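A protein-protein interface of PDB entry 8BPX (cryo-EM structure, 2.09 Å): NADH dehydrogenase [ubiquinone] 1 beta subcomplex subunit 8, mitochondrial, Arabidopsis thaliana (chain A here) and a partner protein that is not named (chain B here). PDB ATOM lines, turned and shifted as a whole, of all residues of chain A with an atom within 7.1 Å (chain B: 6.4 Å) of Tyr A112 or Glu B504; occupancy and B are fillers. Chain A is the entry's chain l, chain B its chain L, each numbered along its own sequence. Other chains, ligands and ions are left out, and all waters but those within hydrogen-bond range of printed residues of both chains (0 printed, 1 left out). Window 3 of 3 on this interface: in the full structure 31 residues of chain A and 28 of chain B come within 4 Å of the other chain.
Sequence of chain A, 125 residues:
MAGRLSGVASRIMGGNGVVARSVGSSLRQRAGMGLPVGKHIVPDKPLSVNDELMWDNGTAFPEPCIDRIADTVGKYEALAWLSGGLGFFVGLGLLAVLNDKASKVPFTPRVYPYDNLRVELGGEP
Of the printed residues of chain A, Glu B504 touches Arg A110 (3.3 Å) and Tyr A112 (3.98 Å). Printed residues of chain B within 4 Å of Phe A107: Glu B508 (3.8 Å). Of the printed residues of chain A, Glu B508 touches Phe A107 (3.8 Å) and Arg A110 (2.7 Å). Printed residues of chain A within 4 Å of Ala B507: Arg A110. Of the printed residues of chain B, Arg A110 touches Glu B504, Ala B507 and Glu B508. Printed residues of chain B within 4 Å of Leu A117: Pro B501. The nearest printed residue of chain B that does not touch Tyr A112 is Lys B502 (4.8 Å). The nearest printed residue of chain A that does not touch Glu B504 is Phe A107 (7.0 Å). The nearest printed residue of chain A that does not touch Ala B507 is Phe A107 (7.5 Å).
The side-chain carboxylate (OE1) of Glu B508 lies within salt-bridge range of the guanidinium group (NH2) of Arg A110, 2.7 Å away.
CE2 of Phe A107 touches CB of Glu B508, at 3.8 Å. Arg A110 touches Glu B504 (NH1 to CB, 3.3 Å). CB of Ala B507 touches NH2 of Arg A110 (3.5 Å). CE1 of Tyr A112 touches CB of Pro B501 (3.3 Å). CB of Glu B504 touches OH of Tyr A112, at 3.98 Å. Pro B501 touches Leu A117 (CG to CD1, 3.96 Å).
OH of Tyr A112 lies within hydrogen-bond range of NH1 of Arg A110, 2.8 Å away. N of Tyr A112 is in hydrogen-bond range of OD1 of Asn A116.
Hydrophobic or aromatic side chains of chain A within 4 Å of the printed part of chain B: Phe A107, Tyr A112 and Leu A117. Printed residues of chain B that touch a printed residue of chain A: Pro B501, Glu B504, Ala B507 and Glu B508. Hydrophobic or aromatic side chains of chain B that line the printed part of chain A: Pro B501 and Ala B507. Among the printed residues, Asp or Glu carboxylates within 4 Å of a Lys or Arg side-chain nitrogen of the other chain: Arg A110 with Glu B508 (2.7 Å).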
ATOM      1  N   PHE A 107      20.075 -11.714 -26.963  1.00  0.00           N
ATOM      2  CA  PHE A 107      20.348 -10.426 -26.347  1.00  0.00           C
ATOM      3  C   PHE A 107      19.126  -9.978 -25.563  1.00  0.00           C
ATOM      4  O   PHE A 107      18.000 -10.381 -25.854  1.00  0.00           O
ATOM      5  CB  PHE A 107      20.741  -9.351 -27.382  1.00  0.00           C
ATOM      6  CG  PHE A 107      19.896  -9.360 -28.623  1.00  0.00           C
ATOM      7  CD1 PHE A 107      18.642  -8.770 -28.633  1.00  0.00           C
ATOM      8  CD2 PHE A 107      20.355  -9.958 -29.781  1.00  0.00           C
ATOM      9  CE1 PHE A 107      17.868  -8.779 -29.776  1.00  0.00           C
ATOM     10  CE2 PHE A 107      19.583  -9.970 -30.925  1.00  0.00           C
ATOM     11  CZ  PHE A 107      18.339  -9.379 -30.919  1.00  0.00           C
ATOM     12  N   PRO A 109      16.446  -7.143 -24.335  1.00  0.00           N
ATOM     13  CA  PRO A 109      15.825  -6.067 -25.100  1.00  0.00           C
ATOM     14  C   PRO A 109      16.550  -4.726 -24.905  1.00  0.00           C
ATOM     15  O   PRO A 109      17.124  -4.528 -23.854  1.00  0.00           O
ATOM     16  CB  PRO A 109      14.357  -6.075 -24.570  1.00  0.00           C
ATOM     17  CG  PRO A 109      14.224  -7.326 -23.770  1.00  0.00           C
ATOM     18  CD  PRO A 109      15.608  -7.624 -23.250  1.00  0.00           C
ATOM     19  N   ARG A 110      16.532  -3.900 -25.963  1.00  0.00           N
ATOM     20  CA  ARG A 110      17.173  -2.562 -25.921  1.00  0.00           C
ATOM     21  C   ARG A 110      16.486  -1.703 -24.872  1.00  0.00           C
ATOM     22  O   ARG A 110      15.278  -1.908 -24.618  1.00  0.00           O
ATOM     23  CB  ARG A 110      17.001  -1.784 -27.229  1.00  0.00           C
ATOM     24  CG  ARG A 110      17.756  -2.333 -28.428  1.00  0.00           C
ATOM     25  CD  ARG A 110      17.636  -1.413 -29.625  1.00  0.00           C
ATOM     26  NE  ARG A 110      18.518  -1.796 -30.717  1.00  0.00           N
ATOM     27  CZ  ARG A 110      18.733  -1.069 -31.806  1.00  0.00           C
ATOM     28  NH1 ARG A 110      18.135   0.101 -31.953  1.00  0.00           N
ATOM     29  NH2 ARG A 110      19.558  -1.502 -32.739  1.00  0.00           N
ATOM     30  N   VAL A 111      17.221  -0.737 -24.338  1.00  0.00           N
ATOM     31  CA  VAL A 111      16.664   0.163 -23.303  1.00  0.00           C
ATOM     32  C   VAL A 111      17.187   1.508 -23.689  1.00  0.00           C
ATOM     33  O   VAL A 111      18.373   1.721 -23.629  1.00  0.00           O
ATOM     34  CB  VAL A 111      16.950  -0.245 -21.843  1.00  0.00           C
ATOM     35  CG1 VAL A 111      16.471   0.822 -20.879  1.00  0.00           C
ATOM     36  CG2 VAL A 111      16.355  -1.593 -21.502  1.00  0.00           C
ATOM     37  N   TYR A 112      16.261   2.341 -24.081  1.00  0.00           N
ATOM     38  CA  TYR A 112      16.618   3.686 -24.506  1.00  0.00           C
ATOM     39  C   TYR A 112      16.770   4.542 -23.265  1.00  0.00           C
ATOM     40  O   TYR A 112      16.119   4.252 -22.307  1.00  0.00           O
ATOM     41  CB  TYR A 112      15.590   4.191 -25.534  1.00  0.00           C
ATOM     42  CG  TYR A 112      15.816   3.571 -26.881  1.00  0.00           C
ATOM     43  CD1 TYR A 112      15.319   2.314 -27.185  1.00  0.00           C
ATOM     44  CD2 TYR A 112      16.591   4.219 -27.819  1.00  0.00           C
ATOM     45  CE1 TYR A 112      15.544   1.747 -28.425  1.00  0.00           C
ATOM     46  CE2 TYR A 112      16.818   3.667 -29.061  1.00  0.00           C
ATOM     47  CZ  TYR A 112      16.287   2.429 -29.364  1.00  0.00           C
ATOM     48  OH  TYR A 112      16.526   1.890 -30.583  1.00  0.00           O
ATOM     49  N   PRO A 113      17.544   5.628 -23.330  1.00  0.00           N
ATOM     50  CA  PRO A 113      17.641   6.589 -22.226  1.00  0.00           C
ATOM     51  C   PRO A 113      16.405   7.465 -22.087  1.00  0.00           C
ATOM     52  O   PRO A 113      15.475   7.391 -22.901  1.00  0.00           O
ATOM     53  CB  PRO A 113      18.873   7.423 -22.598  1.00  0.00           C
ATOM     54  CG  PRO A 113      18.905   7.357 -24.089  1.00  0.00           C
ATOM     55  CD  PRO A 113      18.462   5.965 -24.433  1.00  0.00           C
ATOM     56  N   TYR A 114      16.401   8.292 -21.044  1.00  0.00           N
ATOM     57  CA  TYR A 114      15.336   9.251 -20.758  1.00  0.00           C
ATOM     58  C   TYR A 114      13.978   8.559 -20.663  1.00  0.00           C
ATOM     59  O   TYR A 114      13.017   8.903 -21.351  1.00  0.00           O
ATOM     60  CB  TYR A 114      15.329  10.372 -21.797  1.00  0.00           C
ATOM     61  CG  TYR A 114      16.649  11.097 -21.861  1.00  0.00           C
ATOM     62  CD1 TYR A 114      17.045  11.945 -20.837  1.00  0.00           C
ATOM     63  CD2 TYR A 114      17.510  10.921 -22.934  1.00  0.00           C
ATOM     64  CE1 TYR A 114      18.251  12.601 -20.880  1.00  0.00           C
ATOM     65  CE2 TYR A 114      18.721  11.577 -22.987  1.00  0.00           C
ATOM     66  CZ  TYR A 114      19.084  12.416 -21.956  1.00  0.00           C
ATOM     67  OH  TYR A 114      20.286  13.075 -22.003  1.00  0.00           O
ATOM     68  N   ASP A 115      13.924   7.572 -19.768  1.00  0.00           N
ATOM     69  CA  ASP A 115      12.717   6.795 -19.491  1.00  0.00           C
ATOM     70  C   ASP A 115      12.180   6.156 -20.773  1.00  0.00           C
ATOM     71  O   ASP A 115      10.989   6.216 -21.084  1.00  0.00           O
ATOM     72  CB  ASP A 115      11.664   7.661 -18.795  1.00  0.00           C
ATOM     73  CG  ASP A 115      10.428   6.880 -18.394  1.00  0.00           C
ATOM     74  OD1 ASP A 115       9.318   7.446 -18.467  1.00  0.00           O
ATOM     75  OD2 ASP A 115      10.568   5.700 -18.012  1.00  0.00           O
ATOM     76  N   ASN A 116      13.035   5.496 -21.505  1.00  0.00           N
ATOM     77  CA  ASN A 116      12.668   4.843 -22.782  1.00  0.00           C
ATOM     78  C   ASN A 116      12.086   5.883 -23.775  1.00  0.00           C
ATOM     79  O   ASN A 116      11.264   5.489 -24.507  1.00  0.00           O
ATOM     80  CB  ASN A 116      11.973   3.499 -22.521  1.00  0.00           C
ATOM     81  CG  ASN A 116      12.836   2.323 -22.891  1.00  0.00           C
ATOM     82  OD1 ASN A 116      13.115   2.096 -24.062  1.00  0.00           O
ATOM     83  ND2 ASN A 116      13.283   1.594 -21.887  1.00  0.00           N
ATOM     84  N   LEU A 117      12.698   7.088 -23.844  1.00  0.00           N
ATOM     85  CA  LEU A 117      12.235   8.137 -24.753  1.00  0.00           C
ATOM     86  C   LEU A 117      10.734   8.374 -24.614  1.00  0.00           C
ATOM     87  O   LEU A 117       9.985   8.377 -25.591  1.00  0.00           O
ATOM     88  CB  LEU A 117      12.603   7.810 -26.202  1.00  0.00           C
ATOM     89  CG  LEU A 117      14.070   7.550 -26.541  1.00  0.00           C
ATOM     90  CD1 LEU A 117      14.188   6.940 -27.923  1.00  0.00           C
ATOM     91  CD2 LEU A 117      14.872   8.836 -26.446  1.00  0.00           C
ATOM     92  N   SER B 329       9.294  -4.109 -40.056  1.00  0.00           N
ATOM     93  CA  SER B 329       9.550  -2.721 -39.665  1.00  0.00           C
ATOM     94  C   SER B 329      10.853  -2.175 -40.242  1.00  0.00           C
ATOM     95  O   SER B 329      11.447  -1.254 -39.681  1.00  0.00           O
ATOM     96  CB  SER B 329       9.541  -2.554 -38.142  1.00  0.00           C
ATOM     97  OG  SER B 329       8.227  -2.387 -37.650  1.00  0.00           O
ATOM     98  N   ASN B 330      11.300  -2.708 -41.373  1.00  0.00           N
ATOM     99  CA  ASN B 330      12.508  -2.224 -42.034  1.00  0.00           C
ATOM    100  C   ASN B 330      12.112  -1.693 -43.404  1.00  0.00           C
ATOM    101  O   ASN B 330      12.277  -2.366 -44.422  1.00  0.00           O
ATOM    102  CB  ASN B 330      13.532  -3.334 -42.120  1.00  0.00           C
ATOM    103  CG  ASN B 330      14.300  -3.510 -40.829  1.00  0.00           C
ATOM    104  OD1 ASN B 330      14.112  -4.485 -40.111  1.00  0.00           O
ATOM    105  ND2 ASN B 330      15.168  -2.560 -40.528  1.00  0.00           N
ATOM    106  N   VAL B 499      10.432   4.208 -37.869  1.00  0.00           N
ATOM    107  CA  VAL B 499      10.652   2.966 -37.139  1.00  0.00           C
ATOM    108  C   VAL B 499      10.623   3.312 -35.662  1.00  0.00           C
ATOM    109  O   VAL B 499      11.429   4.126 -35.197  1.00  0.00           O
ATOM    110  CB  VAL B 499      11.981   2.292 -37.517  1.00  0.00           C
ATOM    111  CG1 VAL B 499      12.070   0.897 -36.907  1.00  0.00           C
ATOM    112  CG2 VAL B 499      12.135   2.226 -39.017  1.00  0.00           C
ATOM    113  N   LEU B 500       9.687   2.704 -34.962  1.00  0.00           N
ATOM    114  CA  LEU B 500       9.624   2.885 -33.506  1.00  0.00           C
ATOM    115  C   LEU B 500      10.868   2.260 -32.882  1.00  0.00           C
ATOM    116  O   LEU B 500      11.288   1.202 -33.370  1.00  0.00           O
ATOM    117  CB  LEU B 500       8.352   2.225 -32.982  1.00  0.00           C
ATOM    118  CG  LEU B 500       7.044   2.940 -33.334  1.00  0.00           C
ATOM    119  CD1 LEU B 500       5.839   2.153 -32.859  1.00  0.00           C
ATOM    120  CD2 LEU B 500       7.008   4.351 -32.778  1.00  0.00           C
ATOM    121  N   PRO B 501      11.424   2.827 -31.793  1.00  0.00           N
ATOM    122  CA  PRO B 501      12.607   2.211 -31.103  1.00  0.00           C
ATOM    123  C   PRO B 501      12.475   0.713 -30.801  1.00  0.00           C
ATOM    124  O   PRO B 501      13.338   0.022 -31.174  1.00  0.00           O
ATOM    125  CB  PRO B 501      12.860   3.068 -29.845  1.00  0.00           C
ATOM    126  CG  PRO B 501      12.153   4.382 -30.167  1.00  0.00           C
ATOM    127  CD  PRO B 501      11.059   4.102 -31.181  1.00  0.00           C
ATOM    128  N   LYS B 502      11.372   0.262 -30.234  1.00  0.00           N
ATOM    129  CA  LYS B 502      11.125  -1.160 -29.881  1.00  0.00           C
ATOM    130  C   LYS B 502      11.301  -2.133 -31.069  1.00  0.00           C
ATOM    131  O   LYS B 502      11.483  -3.256 -30.807  1.00  0.00           O
ATOM    132  CB  LYS B 502       9.726  -1.219 -29.269  1.00  0.00           C
ATOM    133  CG  LYS B 502       8.581  -1.242 -30.262  1.00  0.00           C
ATOM    134  CD  LYS B 502       7.269  -0.961 -29.619  1.00  0.00           C
ATOM    135  CE  LYS B 502       6.168  -0.721 -30.622  1.00  0.00           C
ATOM    136  NZ  LYS B 502       5.682  -1.978 -31.220  1.00  0.00           N
ATOM    137  N   ASN B 503      11.207  -1.682 -32.308  1.00  0.00           N
ATOM    138  CA  ASN B 503      11.318  -2.493 -33.547  1.00  0.00           C
ATOM    139  C   ASN B 503      12.666  -2.380 -34.254  1.00  0.00           C
ATOM    140  O   ASN B 503      12.793  -3.002 -35.248  1.00  0.00           O
ATOM    141  CB  ASN B 503      10.170  -2.147 -34.538  1.00  0.00           C
ATOM    142  CG  ASN B 503       8.802  -2.415 -33.962  1.00  0.00           C
ATOM    143  OD1 ASN B 503       8.632  -3.326 -33.162  1.00  0.00           O
ATOM    144  ND2 ASN B 503       7.833  -1.611 -34.350  1.00  0.00           N
ATOM    145  N   GLU B 504      13.551  -1.538 -33.771  1.00  0.00           N
ATOM    146  CA  GLU B 504      14.885  -1.323 -34.391  1.00  0.00           C
ATOM    147  C   GLU B 504      15.776  -2.572 -34.201  1.00  0.00           C
ATOM    148  O   GLU B 504      16.054  -2.940 -33.088  1.00  0.00           O
ATOM    149  CB  GLU B 504      15.477   0.033 -33.947  1.00  0.00           C
ATOM    150  CG  GLU B 504      15.090   1.227 -34.790  1.00  0.00           C
ATOM    151  CD  GLU B 504      15.450   1.278 -36.271  1.00  0.00           C
ATOM    152  OE1 GLU B 504      15.909   0.268 -36.832  1.00  0.00           O
ATOM    153  OE2 GLU B 504      15.258   2.344 -36.867  1.00  0.00           O
ATOM    154  N   ILE B 505      16.180  -3.197 -35.274  1.00  0.00           N
ATOM    155  CA  ILE B 505      16.996  -4.441 -35.275  1.00  0.00           C
ATOM    156  C   ILE B 505      18.213  -4.354 -36.200  1.00  0.00           C
ATOM    157  O   ILE B 505      18.896  -5.346 -36.273  1.00  0.00           O
ATOM    158  CB  ILE B 505      16.130  -5.671 -35.689  1.00  0.00           C
ATOM    159  CG1 ILE B 505      15.532  -5.522 -37.088  1.00  0.00           C
ATOM    160  CG2 ILE B 505      15.057  -6.002 -34.658  1.00  0.00           C
ATOM    161  CD1 ILE B 505      14.837  -6.767 -37.578  1.00  0.00           C
ATOM    162  N   LEU B 506      18.481  -3.262 -36.872  1.00  0.00           N
ATOM    163  CA  LEU B 506      19.587  -3.227 -37.858  1.00  0.00           C
ATOM    164  C   LEU B 506      20.987  -3.497 -37.203  1.00  0.00           C
ATOM    165  O   LEU B 506      21.694  -4.329 -37.757  1.00  0.00           O
ATOM    166  CB  LEU B 506      19.560  -1.940 -38.639  1.00  0.00           C
ATOM    167  CG  LEU B 506      20.551  -1.848 -39.800  1.00  0.00           C
ATOM    168  CD1 LEU B 506      20.229  -2.842 -40.909  1.00  0.00           C
ATOM    169  CD2 LEU B 506      20.624  -0.434 -40.343  1.00  0.00           C
ATOM    170  N   ALA B 507      21.334  -2.882 -36.081  1.00  0.00           N
ATOM    171  CA  ALA B 507      22.618  -3.114 -35.345  1.00  0.00           C
ATOM    172  C   ALA B 507      22.789  -4.588 -35.005  1.00  0.00           C
ATOM    173  O   ALA B 507      23.760  -5.137 -35.446  1.00  0.00           O
ATOM    174  CB  ALA B 507      22.680  -2.252 -34.114  1.00  0.00           C
ATOM    175  N   GLU B 508      21.806  -5.188 -34.349  1.00  0.00           N
ATOM    176  CA  GLU B 508      21.836  -6.603 -33.939  1.00  0.00           C
ATOM    177  C   GLU B 508      21.981  -7.518 -35.170  1.00  0.00           C
ATOM    178  O   GLU B 508      22.579  -8.557 -35.008  1.00  0.00           O
ATOM    179  CB  GLU B 508      20.634  -6.930 -33.028  1.00  0.00           C
ATOM    180  CG  GLU B 508      20.445  -6.020 -31.843  1.00  0.00           C
ATOM    181  CD  GLU B 508      19.427  -4.910 -32.030  1.00  0.00           C
ATOM    182  OE1 GLU B 508      19.496  -4.205 -33.037  1.00  0.00           O
ATOM    183  OE2 GLU B 508      18.579  -4.757 -31.166  1.00  0.00           O
